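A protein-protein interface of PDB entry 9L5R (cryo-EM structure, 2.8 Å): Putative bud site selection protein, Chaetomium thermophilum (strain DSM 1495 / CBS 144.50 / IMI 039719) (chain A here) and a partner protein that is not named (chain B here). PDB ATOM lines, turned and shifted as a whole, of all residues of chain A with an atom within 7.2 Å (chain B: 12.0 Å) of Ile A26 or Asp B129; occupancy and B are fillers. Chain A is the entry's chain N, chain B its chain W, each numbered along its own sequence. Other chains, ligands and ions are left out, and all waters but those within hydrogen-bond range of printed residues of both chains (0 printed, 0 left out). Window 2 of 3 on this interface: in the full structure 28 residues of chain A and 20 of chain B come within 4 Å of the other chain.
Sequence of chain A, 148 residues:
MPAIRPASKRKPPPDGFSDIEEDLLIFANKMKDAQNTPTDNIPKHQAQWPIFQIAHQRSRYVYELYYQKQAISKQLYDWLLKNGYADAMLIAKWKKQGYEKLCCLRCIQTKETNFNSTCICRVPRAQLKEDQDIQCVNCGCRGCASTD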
ATOM      1  N   ILE A  20      22.628   0.418   6.791  1.00  0.00           N
ATOM      2  CA  ILE A  20      22.305  -1.008   6.716  1.00  0.00           C
ATOM      3  C   ILE A  20      22.281  -1.544   5.296  1.00  0.00           C
ATOM      4  O   ILE A  20      22.047  -2.755   5.105  1.00  0.00           O
ATOM      5  CB  ILE A  20      20.970  -1.316   7.416  1.00  0.00           C
ATOM      6  CG1 ILE A  20      19.849  -0.500   6.791  1.00  0.00           C
ATOM      7  CG2 ILE A  20      21.073  -1.008   8.875  1.00  0.00           C
ATOM      8  CD1 ILE A  20      18.512  -0.796   7.377  1.00  0.00           C
ATOM      9  N   GLU A  21      22.531  -0.696   4.295  1.00  0.00           N
ATOM     10  CA  GLU A  21      22.388  -1.091   2.900  1.00  0.00           C
ATOM     11  C   GLU A  21      23.344  -2.203   2.504  1.00  0.00           C
ATOM     12  O   GLU A  21      23.004  -3.027   1.653  1.00  0.00           O
ATOM     13  CB  GLU A  21      22.602   0.128   2.008  1.00  0.00           C
ATOM     14  CG  GLU A  21      22.081  -0.014   0.599  1.00  0.00           C
ATOM     15  CD  GLU A  21      22.213   1.273  -0.187  1.00  0.00           C
ATOM     16  OE1 GLU A  21      23.090   2.087   0.158  1.00  0.00           O
ATOM     17  OE2 GLU A  21      21.439   1.472  -1.145  1.00  0.00           O
ATOM     18  N   GLU A  22      24.525  -2.260   3.115  1.00  0.00           N
ATOM     19  CA  GLU A  22      25.493  -3.284   2.740  1.00  0.00           C
ATOM     20  C   GLU A  22      25.029  -4.672   3.157  1.00  0.00           C
ATOM     21  O   GLU A  22      25.118  -5.623   2.372  1.00  0.00           O
ATOM     22  CB  GLU A  22      26.854  -2.961   3.350  1.00  0.00           C
ATOM     23  CG  GLU A  22      27.704  -2.068   2.469  1.00  0.00           C
ATOM     24  CD  GLU A  22      27.238  -0.623   2.470  1.00  0.00           C
ATOM     25  OE1 GLU A  22      26.450  -0.243   3.360  1.00  0.00           O
ATOM     26  OE2 GLU A  22      27.657   0.134   1.571  1.00  0.00           O
ATOM     27  N   ASP A  23      24.506  -4.806   4.375  1.00  0.00           N
ATOM     28  CA  ASP A  23      23.981  -6.096   4.805  1.00  0.00           C
ATOM     29  C   ASP A  23      22.716  -6.460   4.042  1.00  0.00           C
ATOM     30  O   ASP A  23      22.503  -7.635   3.711  1.00  0.00           O
ATOM     31  CB  ASP A  23      23.717  -6.080   6.303  1.00  0.00           C
ATOM     32  CG  ASP A  23      24.982  -5.931   7.111  1.00  0.00           C
ATOM     33  OD1 ASP A  23      25.399  -4.780   7.345  1.00  0.00           O
ATOM     34  OD2 ASP A  23      25.561  -6.960   7.515  1.00  0.00           O
ATOM     35  N   LEU A  24      21.873  -5.466   3.739  1.00  0.00           N
ATOM     36  CA  LEU A  24      20.678  -5.750   2.947  1.00  0.00           C
ATOM     37  C   LEU A  24      21.040  -6.244   1.550  1.00  0.00           C
ATOM     38  O   LEU A  24      20.422  -7.183   1.037  1.00  0.00           O
ATOM     39  CB  LEU A  24      19.788  -4.513   2.873  1.00  0.00           C
ATOM     40  CG  LEU A  24      19.162  -4.032   4.185  1.00  0.00           C
ATOM     41  CD1 LEU A  24      18.087  -3.022   3.907  1.00  0.00           C
ATOM     42  CD2 LEU A  24      18.606  -5.178   4.997  1.00  0.00           C
ATOM     43  N   LEU A  25      22.064  -5.651   0.933  1.00  0.00           N
ATOM     44  CA  LEU A  25      22.512  -6.116  -0.375  1.00  0.00           C
ATOM     45  C   LEU A  25      23.209  -7.463  -0.294  1.00  0.00           C
ATOM     46  O   LEU A  25      23.170  -8.229  -1.261  1.00  0.00           O
ATOM     47  CB  LEU A  25      23.433  -5.087  -1.019  1.00  0.00           C
ATOM     48  CG  LEU A  25      22.808  -4.121  -2.025  1.00  0.00           C
ATOM     49  CD1 LEU A  25      21.756  -3.240  -1.396  1.00  0.00           C
ATOM     50  CD2 LEU A  25      23.899  -3.265  -2.624  1.00  0.00           C
ATOM     51  N   ILE A  26      23.855  -7.767   0.835  1.00  0.00           N
ATOM     52  CA  ILE A  26      24.420  -9.100   1.031  1.00  0.00           C
ATOM     53  C   ILE A  26      23.314 -10.145   1.008  1.00  0.00           C
ATOM     54  O   ILE A  26      23.425 -11.180   0.339  1.00  0.00           O
ATOM     55  CB  ILE A  26      25.225  -9.154   2.341  1.00  0.00           C
ATOM     56  CG1 ILE A  26      26.602  -8.529   2.151  1.00  0.00           C
ATOM     57  CG2 ILE A  26      25.394 -10.578   2.825  1.00  0.00           C
ATOM     58  CD1 ILE A  26      27.343  -8.320   3.445  1.00  0.00           C
ATOM     59  N   PHE A  27      22.214  -9.866   1.711  1.00  0.00           N
ATOM     60  CA  PHE A  27      21.070 -10.776   1.694  1.00  0.00           C
ATOM     61  C   PHE A  27      20.439 -10.868   0.307  1.00  0.00           C
ATOM     62  O   PHE A  27      20.028 -11.951  -0.124  1.00  0.00           O
ATOM     63  CB  PHE A  27      20.035 -10.338   2.720  1.00  0.00           C
ATOM     64  CG  PHE A  27      20.415 -10.660   4.126  1.00  0.00           C
ATOM     65  CD1 PHE A  27      20.659 -11.962   4.503  1.00  0.00           C
ATOM     66  CD2 PHE A  27      20.530  -9.663   5.072  1.00  0.00           C
ATOM     67  CE1 PHE A  27      21.012 -12.258   5.792  1.00  0.00           C
ATOM     68  CE2 PHE A  27      20.881  -9.957   6.357  1.00  0.00           C
ATOM     69  CZ  PHE A  27      21.121 -11.256   6.719  1.00  0.00           C
ATOM     70  N   ALA A  28      20.358  -9.745  -0.406  1.00  0.00           N
ATOM     71  CA  ALA A  28      19.770  -9.760  -1.742  1.00  0.00           C
ATOM     72  C   ALA A  28      20.602 -10.583  -2.721  1.00  0.00           C
ATOM     73  O   ALA A  28      20.054 -11.343  -3.532  1.00  0.00           O
ATOM     74  CB  ALA A  28      19.603  -8.332  -2.249  1.00  0.00           C
ATOM     75  N   ASN A  29      21.926 -10.458  -2.657  1.00  0.00           N
ATOM     76  CA  ASN A  29      22.764 -11.238  -3.556  1.00  0.00           C
ATOM     77  C   ASN A  29      22.783 -12.701  -3.159  1.00  0.00           C
ATOM     78  O   ASN A  29      22.873 -13.574  -4.028  1.00  0.00           O
ATOM     79  CB  ASN A  29      24.174 -10.666  -3.590  1.00  0.00           C
ATOM     80  CG  ASN A  29      24.229  -9.334  -4.286  1.00  0.00           C
ATOM     81  OD1 ASN A  29      23.249  -8.899  -4.881  1.00  0.00           O
ATOM     82  ND2 ASN A  29      25.372  -8.680  -4.221  1.00  0.00           N
ATOM     83  N   LYS A  30      22.670 -12.985  -1.862  1.00  0.00           N
ATOM     84  CA  LYS A  30      22.509 -14.359  -1.407  1.00  0.00           C
ATOM     85  C   LYS A  30      21.236 -14.969  -1.972  1.00  0.00           C
ATOM     86  O   LYS A  30      21.214 -16.139  -2.374  1.00  0.00           O
ATOM     87  CB  LYS A  30      22.486 -14.372   0.117  1.00  0.00           C
ATOM     88  CG  LYS A  30      22.768 -15.693   0.758  1.00  0.00           C
ATOM     89  CD  LYS A  30      22.670 -15.558   2.260  1.00  0.00           C
ATOM     90  CE  LYS A  30      23.733 -14.634   2.784  1.00  0.00           C
ATOM     91  NZ  LYS A  30      25.076 -15.251   2.649  1.00  0.00           N
ATOM     92  N   MET A  31      20.170 -14.172  -2.034  1.00  0.00           N
ATOM     93  CA  MET A  31      18.904 -14.645  -2.575  1.00  0.00           C
ATOM     94  C   MET A  31      18.992 -14.891  -4.078  1.00  0.00           C
ATOM     95  O   MET A  31      18.434 -15.870  -4.588  1.00  0.00           O
ATOM     96  CB  MET A  31      17.810 -13.638  -2.244  1.00  0.00           C
ATOM     97  CG  MET A  31      16.453 -14.081  -2.649  1.00  0.00           C
ATOM     98  SD  MET A  31      15.815 -15.555  -1.829  1.00  0.00           S
ATOM     99  CE  MET A  31      15.456 -14.931  -0.211  1.00  0.00           C
ATOM    100  N   LYS A  32      19.699 -14.028  -4.802  1.00  0.00           N
ATOM    101  CA  LYS A  32      19.897 -14.271  -6.231  1.00  0.00           C
ATOM    102  C   LYS A  32      20.754 -15.513  -6.483  1.00  0.00           C
ATOM    103  O   LYS A  32      20.521 -16.255  -7.447  1.00  0.00           O
ATOM    104  CB  LYS A  32      20.513 -13.046  -6.891  1.00  0.00           C
ATOM    105  CG  LYS A  32      19.529 -11.920  -7.089  1.00  0.00           C
ATOM    106  CD  LYS A  32      20.131 -10.804  -7.899  1.00  0.00           C
ATOM    107  CE  LYS A  32      19.188  -9.630  -7.985  1.00  0.00           C
ATOM    108  NZ  LYS A  32      18.901  -9.045  -6.649  1.00  0.00           N
ATOM    109  N   ASP A  33      21.747 -15.765  -5.629  1.00  0.00           N
ATOM    110  CA  ASP A  33      22.534 -16.985  -5.777  1.00  0.00           C
ATOM    111  C   ASP A  33      21.699 -18.223  -5.482  1.00  0.00           C
ATOM    112  O   ASP A  33      21.889 -19.273  -6.111  1.00  0.00           O
ATOM    113  CB  ASP A  33      23.759 -16.937  -4.870  1.00  0.00           C
ATOM    114  CG  ASP A  33      24.664 -15.780  -5.190  1.00  0.00           C
ATOM    115  OD1 ASP A  33      24.521 -15.203  -6.288  1.00  0.00           O
ATOM    116  OD2 ASP A  33      25.518 -15.439  -4.345  1.00  0.00           O
ATOM    117  N   ILE A  54      17.091 -18.135   3.535  1.00  0.00           N
ATOM    118  CA  ILE A  54      17.571 -16.765   3.379  1.00  0.00           C
ATOM    119  C   ILE A  54      16.494 -15.753   3.745  1.00  0.00           C
ATOM    120  O   ILE A  54      16.802 -14.690   4.293  1.00  0.00           O
ATOM    121  CB  ILE A  54      18.099 -16.564   1.950  1.00  0.00           C
ATOM    122  CG1 ILE A  54      19.252 -17.516   1.708  1.00  0.00           C
ATOM    123  CG2 ILE A  54      18.595 -15.160   1.726  1.00  0.00           C
ATOM    124  CD1 ILE A  54      19.513 -17.752   0.300  1.00  0.00           C
ATOM    125  N   ASP B 121      25.943 -24.093  16.775  1.00  0.00           N
ATOM    126  CA  ASP B 121      25.756 -22.683  17.083  1.00  0.00           C
ATOM    127  C   ASP B 121      24.841 -22.025  16.059  1.00  0.00           C
ATOM    128  O   ASP B 121      25.062 -22.145  14.852  1.00  0.00           O
ATOM    129  CB  ASP B 121      27.112 -21.983  17.112  1.00  0.00           C
ATOM    130  CG  ASP B 121      27.011 -20.531  17.496  1.00  0.00           C
ATOM    131  OD1 ASP B 121      26.376 -20.227  18.528  1.00  0.00           O
ATOM    132  OD2 ASP B 121      27.579 -19.689  16.771  1.00  0.00           O
ATOM    133  N   LYS B 122      23.817 -21.321  16.547  1.00  0.00           N
ATOM    134  CA  LYS B 122      22.831 -20.721  15.652  1.00  0.00           C
ATOM    135  C   LYS B 122      23.394 -19.509  14.923  1.00  0.00           C
ATOM    136  O   LYS B 122      22.999 -19.226  13.789  1.00  0.00           O
ATOM    137  CB  LYS B 122      21.584 -20.322  16.432  1.00  0.00           C
ATOM    138  CG  LYS B 122      21.114 -21.340  17.436  1.00  0.00           C
ATOM    139  CD  LYS B 122      20.552 -22.570  16.772  1.00  0.00           C
ATOM    140  CE  LYS B 122      19.683 -23.344  17.734  1.00  0.00           C
ATOM    141  NZ  LYS B 122      18.473 -22.572  18.106  1.00  0.00           N
ATOM    142  N   GLY B 123      24.289 -18.771  15.555  1.00  0.00           N
ATOM    143  CA  GLY B 123      24.793 -17.536  14.992  1.00  0.00           C
ATOM    144  C   GLY B 123      24.134 -16.328  15.633  1.00  0.00           C
ATOM    145  O   GLY B 123      23.298 -16.438  16.529  1.00  0.00           O
ATOM    146  N   SER B 124      24.515 -15.155  15.130  1.00  0.00           N
ATOM    147  CA  SER B 124      24.220 -13.902  15.811  1.00  0.00           C
ATOM    148  C   SER B 124      23.037 -13.135  15.241  1.00  0.00           C
ATOM    149  O   SER B 124      22.428 -12.352  15.978  1.00  0.00           O
ATOM    150  CB  SER B 124      25.437 -12.984  15.768  1.00  0.00           C
ATOM    151  OG  SER B 124      25.543 -12.415  14.482  1.00  0.00           O
ATOM    152  N   ALA B 125      22.734 -13.299  13.954  1.00  0.00           N
ATOM    153  CA  ALA B 125      21.626 -12.666  13.238  1.00  0.00           C
ATOM    154  C   ALA B 125      21.705 -11.152  13.192  1.00  0.00           C
ATOM    155  O   ALA B 125      20.693 -10.501  12.950  1.00  0.00           O
ATOM    156  CB  ALA B 125      20.261 -13.080  13.792  1.00  0.00           C
ATOM    157  N   THR B 126      22.872 -10.574  13.432  1.00  0.00           N
ATOM    158  CA  THR B 126      23.158  -9.211  13.028  1.00  0.00           C
ATOM    159  C   THR B 126      24.398  -9.159  12.161  1.00  0.00           C
ATOM    160  O   THR B 126      24.762  -8.083  11.678  1.00  0.00           O
ATOM    161  CB  THR B 126      23.323  -8.300  14.247  1.00  0.00           C
ATOM    162  OG1 THR B 126      24.104  -8.966  15.244  1.00  0.00           O
ATOM    163  CG2 THR B 126      21.969  -7.951  14.826  1.00  0.00           C
ATOM    164  N   ILE B 127      25.051 -10.295  11.955  1.00  0.00           N
ATOM    165  CA  ILE B 127      26.132 -10.445  10.996  1.00  0.00           C
ATOM    166  C   ILE B 127      25.545 -11.162   9.791  1.00  0.00           C
ATOM    167  O   ILE B 127      25.135 -12.322   9.888  1.00  0.00           O
ATOM    168  CB  ILE B 127      27.309 -11.223  11.592  1.00  0.00           C
ATOM    169  CG1 ILE B 127      27.719 -10.623  12.935  1.00  0.00           C
ATOM    170  CG2 ILE B 127      28.486 -11.189  10.660  1.00  0.00           C
ATOM    171  CD1 ILE B 127      28.623 -11.524  13.745  1.00  0.00           C
ATOM    172  N   ALA B 128      25.493 -10.476   8.650  1.00  0.00           N
ATOM    173  CA  ALA B 128      24.830 -11.045   7.485  1.00  0.00           C
ATOM    174  C   ALA B 128      25.659 -12.147   6.844  1.00  0.00           C
ATOM    175  O   ALA B 128      25.116 -13.178   6.434  1.00  0.00           O
ATOM    176  CB  ALA B 128      24.532  -9.950   6.464  1.00  0.00           C
ATOM    177  N   ASP B 129      26.968 -11.957   6.744  1.00  0.00           N
ATOM    178  CA  ASP B 129      27.808 -12.841   5.957  1.00  0.00           C
ATOM    179  C   ASP B 129      28.981 -13.322   6.800  1.00  0.00           C
ATOM    180  O   ASP B 129      29.160 -12.914   7.948  1.00  0.00           O
ATOM    181  CB  ASP B 129      28.304 -12.137   4.688  1.00  0.00           C
ATOM    182  CG  ASP B 129      28.484 -13.090   3.523  1.00  0.00           C
ATOM    183  OD1 ASP B 129      28.204 -14.295   3.695  1.00  0.00           O
ATOM    184  OD2 ASP B 129      28.901 -12.634   2.438  1.00  0.00           O
ATOM    185  N   GLY B 130      29.775 -14.210   6.217  1.00  0.00           N
ATOM    186  CA  GLY B 130      30.977 -14.678   6.869  1.00  0.00           C
ATOM    187  C   GLY B 130      30.692 -15.616   8.027  1.00  0.00           C
ATOM    188  O   GLY B 130      29.618 -16.206   8.149  1.00  0.00           O
ATOM    189  N   GLU B 131      31.693 -15.754   8.890  1.00  0.00           N
ATOM    190  CA  GLU B 131      31.558 -16.609  10.057  1.00  0.00           C
ATOM    191  C   GLU B 131      30.760 -15.884  11.133  1.00  0.00           C
ATOM    192  O   GLU B 131      30.828 -14.659  11.255  1.00  0.00           O
ATOM    193  CB  GLU B 131      32.941 -17.010  10.572  1.00  0.00           C
ATOM    194  CG  GLU B 131      32.943 -17.976  11.744  1.00  0.00           C
ATOM    195  CD  GLU B 131      34.336 -18.372  12.171  1.00  0.00           C
ATOM    196  OE1 GLU B 131      35.308 -17.876  11.565  1.00  0.00           O
ATOM    197  OE2 GLU B 131      34.460 -19.187  13.106  1.00  0.00           O
ATOM    198  N   GLY B 132      29.987 -16.642  11.903  1.00  0.00           N
ATOM    199  CA  GLY B 132      29.115 -16.077  12.904  1.00  0.00           C
ATOM    200  C   GLY B 132      27.738 -15.704  12.410  1.00  0.00           C
ATOM    201  O   GLY B 132      26.924 -15.227  13.208  1.00  0.00           O
ATOM    202  N   ALA B 133      27.449 -15.915  11.129  1.00  0.00           N
ATOM    203  CA  ALA B 133      26.157 -15.559  10.566  1.00  0.00           C
ATOM    204  C   ALA B 133      25.060 -16.462  11.114  1.00  0.00           C
ATOM    205  O   ALA B 133      25.313 -17.541  11.653  1.00  0.00           O
ATOM    206  CB  ALA B 133      26.188 -15.652   9.045  1.00  0.00           C
ATOM    207  N   TYR B 134      23.826 -15.996  10.974  1.00  0.00           N
ATOM    208  CA  TYR B 134      22.686 -16.711  11.524  1.00  0.00           C
ATOM    209  C   TYR B 134      22.385 -17.946  10.694  1.00  0.00           C
ATOM    210  O   TYR B 134      22.324 -17.879   9.466  1.00  0.00           O
ATOM    211  CB  TYR B 134      21.470 -15.796  11.558  1.00  0.00           C
ATOM    212  CG  TYR B 134      20.301 -16.325  12.338  1.00  0.00           C
ATOM    213  CD1 TYR B 134      20.426 -16.648  13.670  1.00  0.00           C
ATOM    214  CD2 TYR B 134      19.070 -16.494  11.741  1.00  0.00           C
ATOM    215  CE1 TYR B 134      19.360 -17.133  14.382  1.00  0.00           C
ATOM    216  CE2 TYR B 134      18.006 -16.985  12.442  1.00  0.00           C
ATOM    217  CZ  TYR B 134      18.149 -17.295  13.761  1.00  0.00           C
ATOM    218  OH  TYR B 134      17.078 -17.784  14.465  1.00  0.00           O
ATOM    219  N   ILE B 135      22.219 -19.082  11.362  1.00  0.00           N
ATOM    220  CA  ILE B 135      21.646 -20.255  10.721  1.00  0.00           C
ATOM    221  C   ILE B 135      20.386 -20.743  11.416  1.00  0.00           C
ATOM    222  O   ILE B 135      19.562 -21.402  10.764  1.00  0.00           O
ATOM    223  CB  ILE B 135      22.672 -21.401  10.601  1.00  0.00           C
ATOM    224  CG1 ILE B 135      23.118 -21.893  11.965  1.00  0.00           C
ATOM    225  CG2 ILE B 135      23.883 -20.952   9.826  1.00  0.00           C
ATOM    226  CD1 ILE B 135      23.976 -23.110  11.886  1.00  0.00           C
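The side-chain carboxylate of Asp B129 lies within salt-bridge range of the side-chain amino group of Lys A30 (3.4 Å).
Among the printed residues, merely in contact across the chains: Asp A23 with Ala B128 (3.3 Å), Phe A27 with Ala B128 (3.7 Å), Ile A26 with Asp B129 (3.8 Å) and Ile A26 with Ala B128 (3.8 Å).
Leu A24 touches none of the printed residues of chain B.
Of chain B, only Ala B128 and Asp B129 come within 4 Å of Ile A26.
No residue of chain B comes within 4 Å of Asn A29.
Of chain B, only Asp B129 (3.4 Å) comes within 4 Å of Lys A30.
Asp A33 touches none of the printed residues of chain B.
Of the printed residues of chain A, Ala B128 touches Asp A23, Ile A26 and Phe A27.
Of chain A, only Ile A26 and Lys A30 come within 4 Å of Asp B129.
The nearest residue of chain B that does not touch Ile A26 is Gly B130 (6.6 Å).
The nearest residue of chain A that does not touch Asp B129 is Asp A23 (5.2 Å).
Of the 15 printed residues of chain B, 2 touch a printed residue of chain A.
Hydrophobic or aromatic side chains of chain B within 4 Å of the printed part of chain A: Ala B128.
Among the printed residues, Asp or Glu carboxylates within 4 Å of a Lys or Arg side-chain nitrogen of the other chain: Lys A30 with Asp B129 (3.4 Å).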
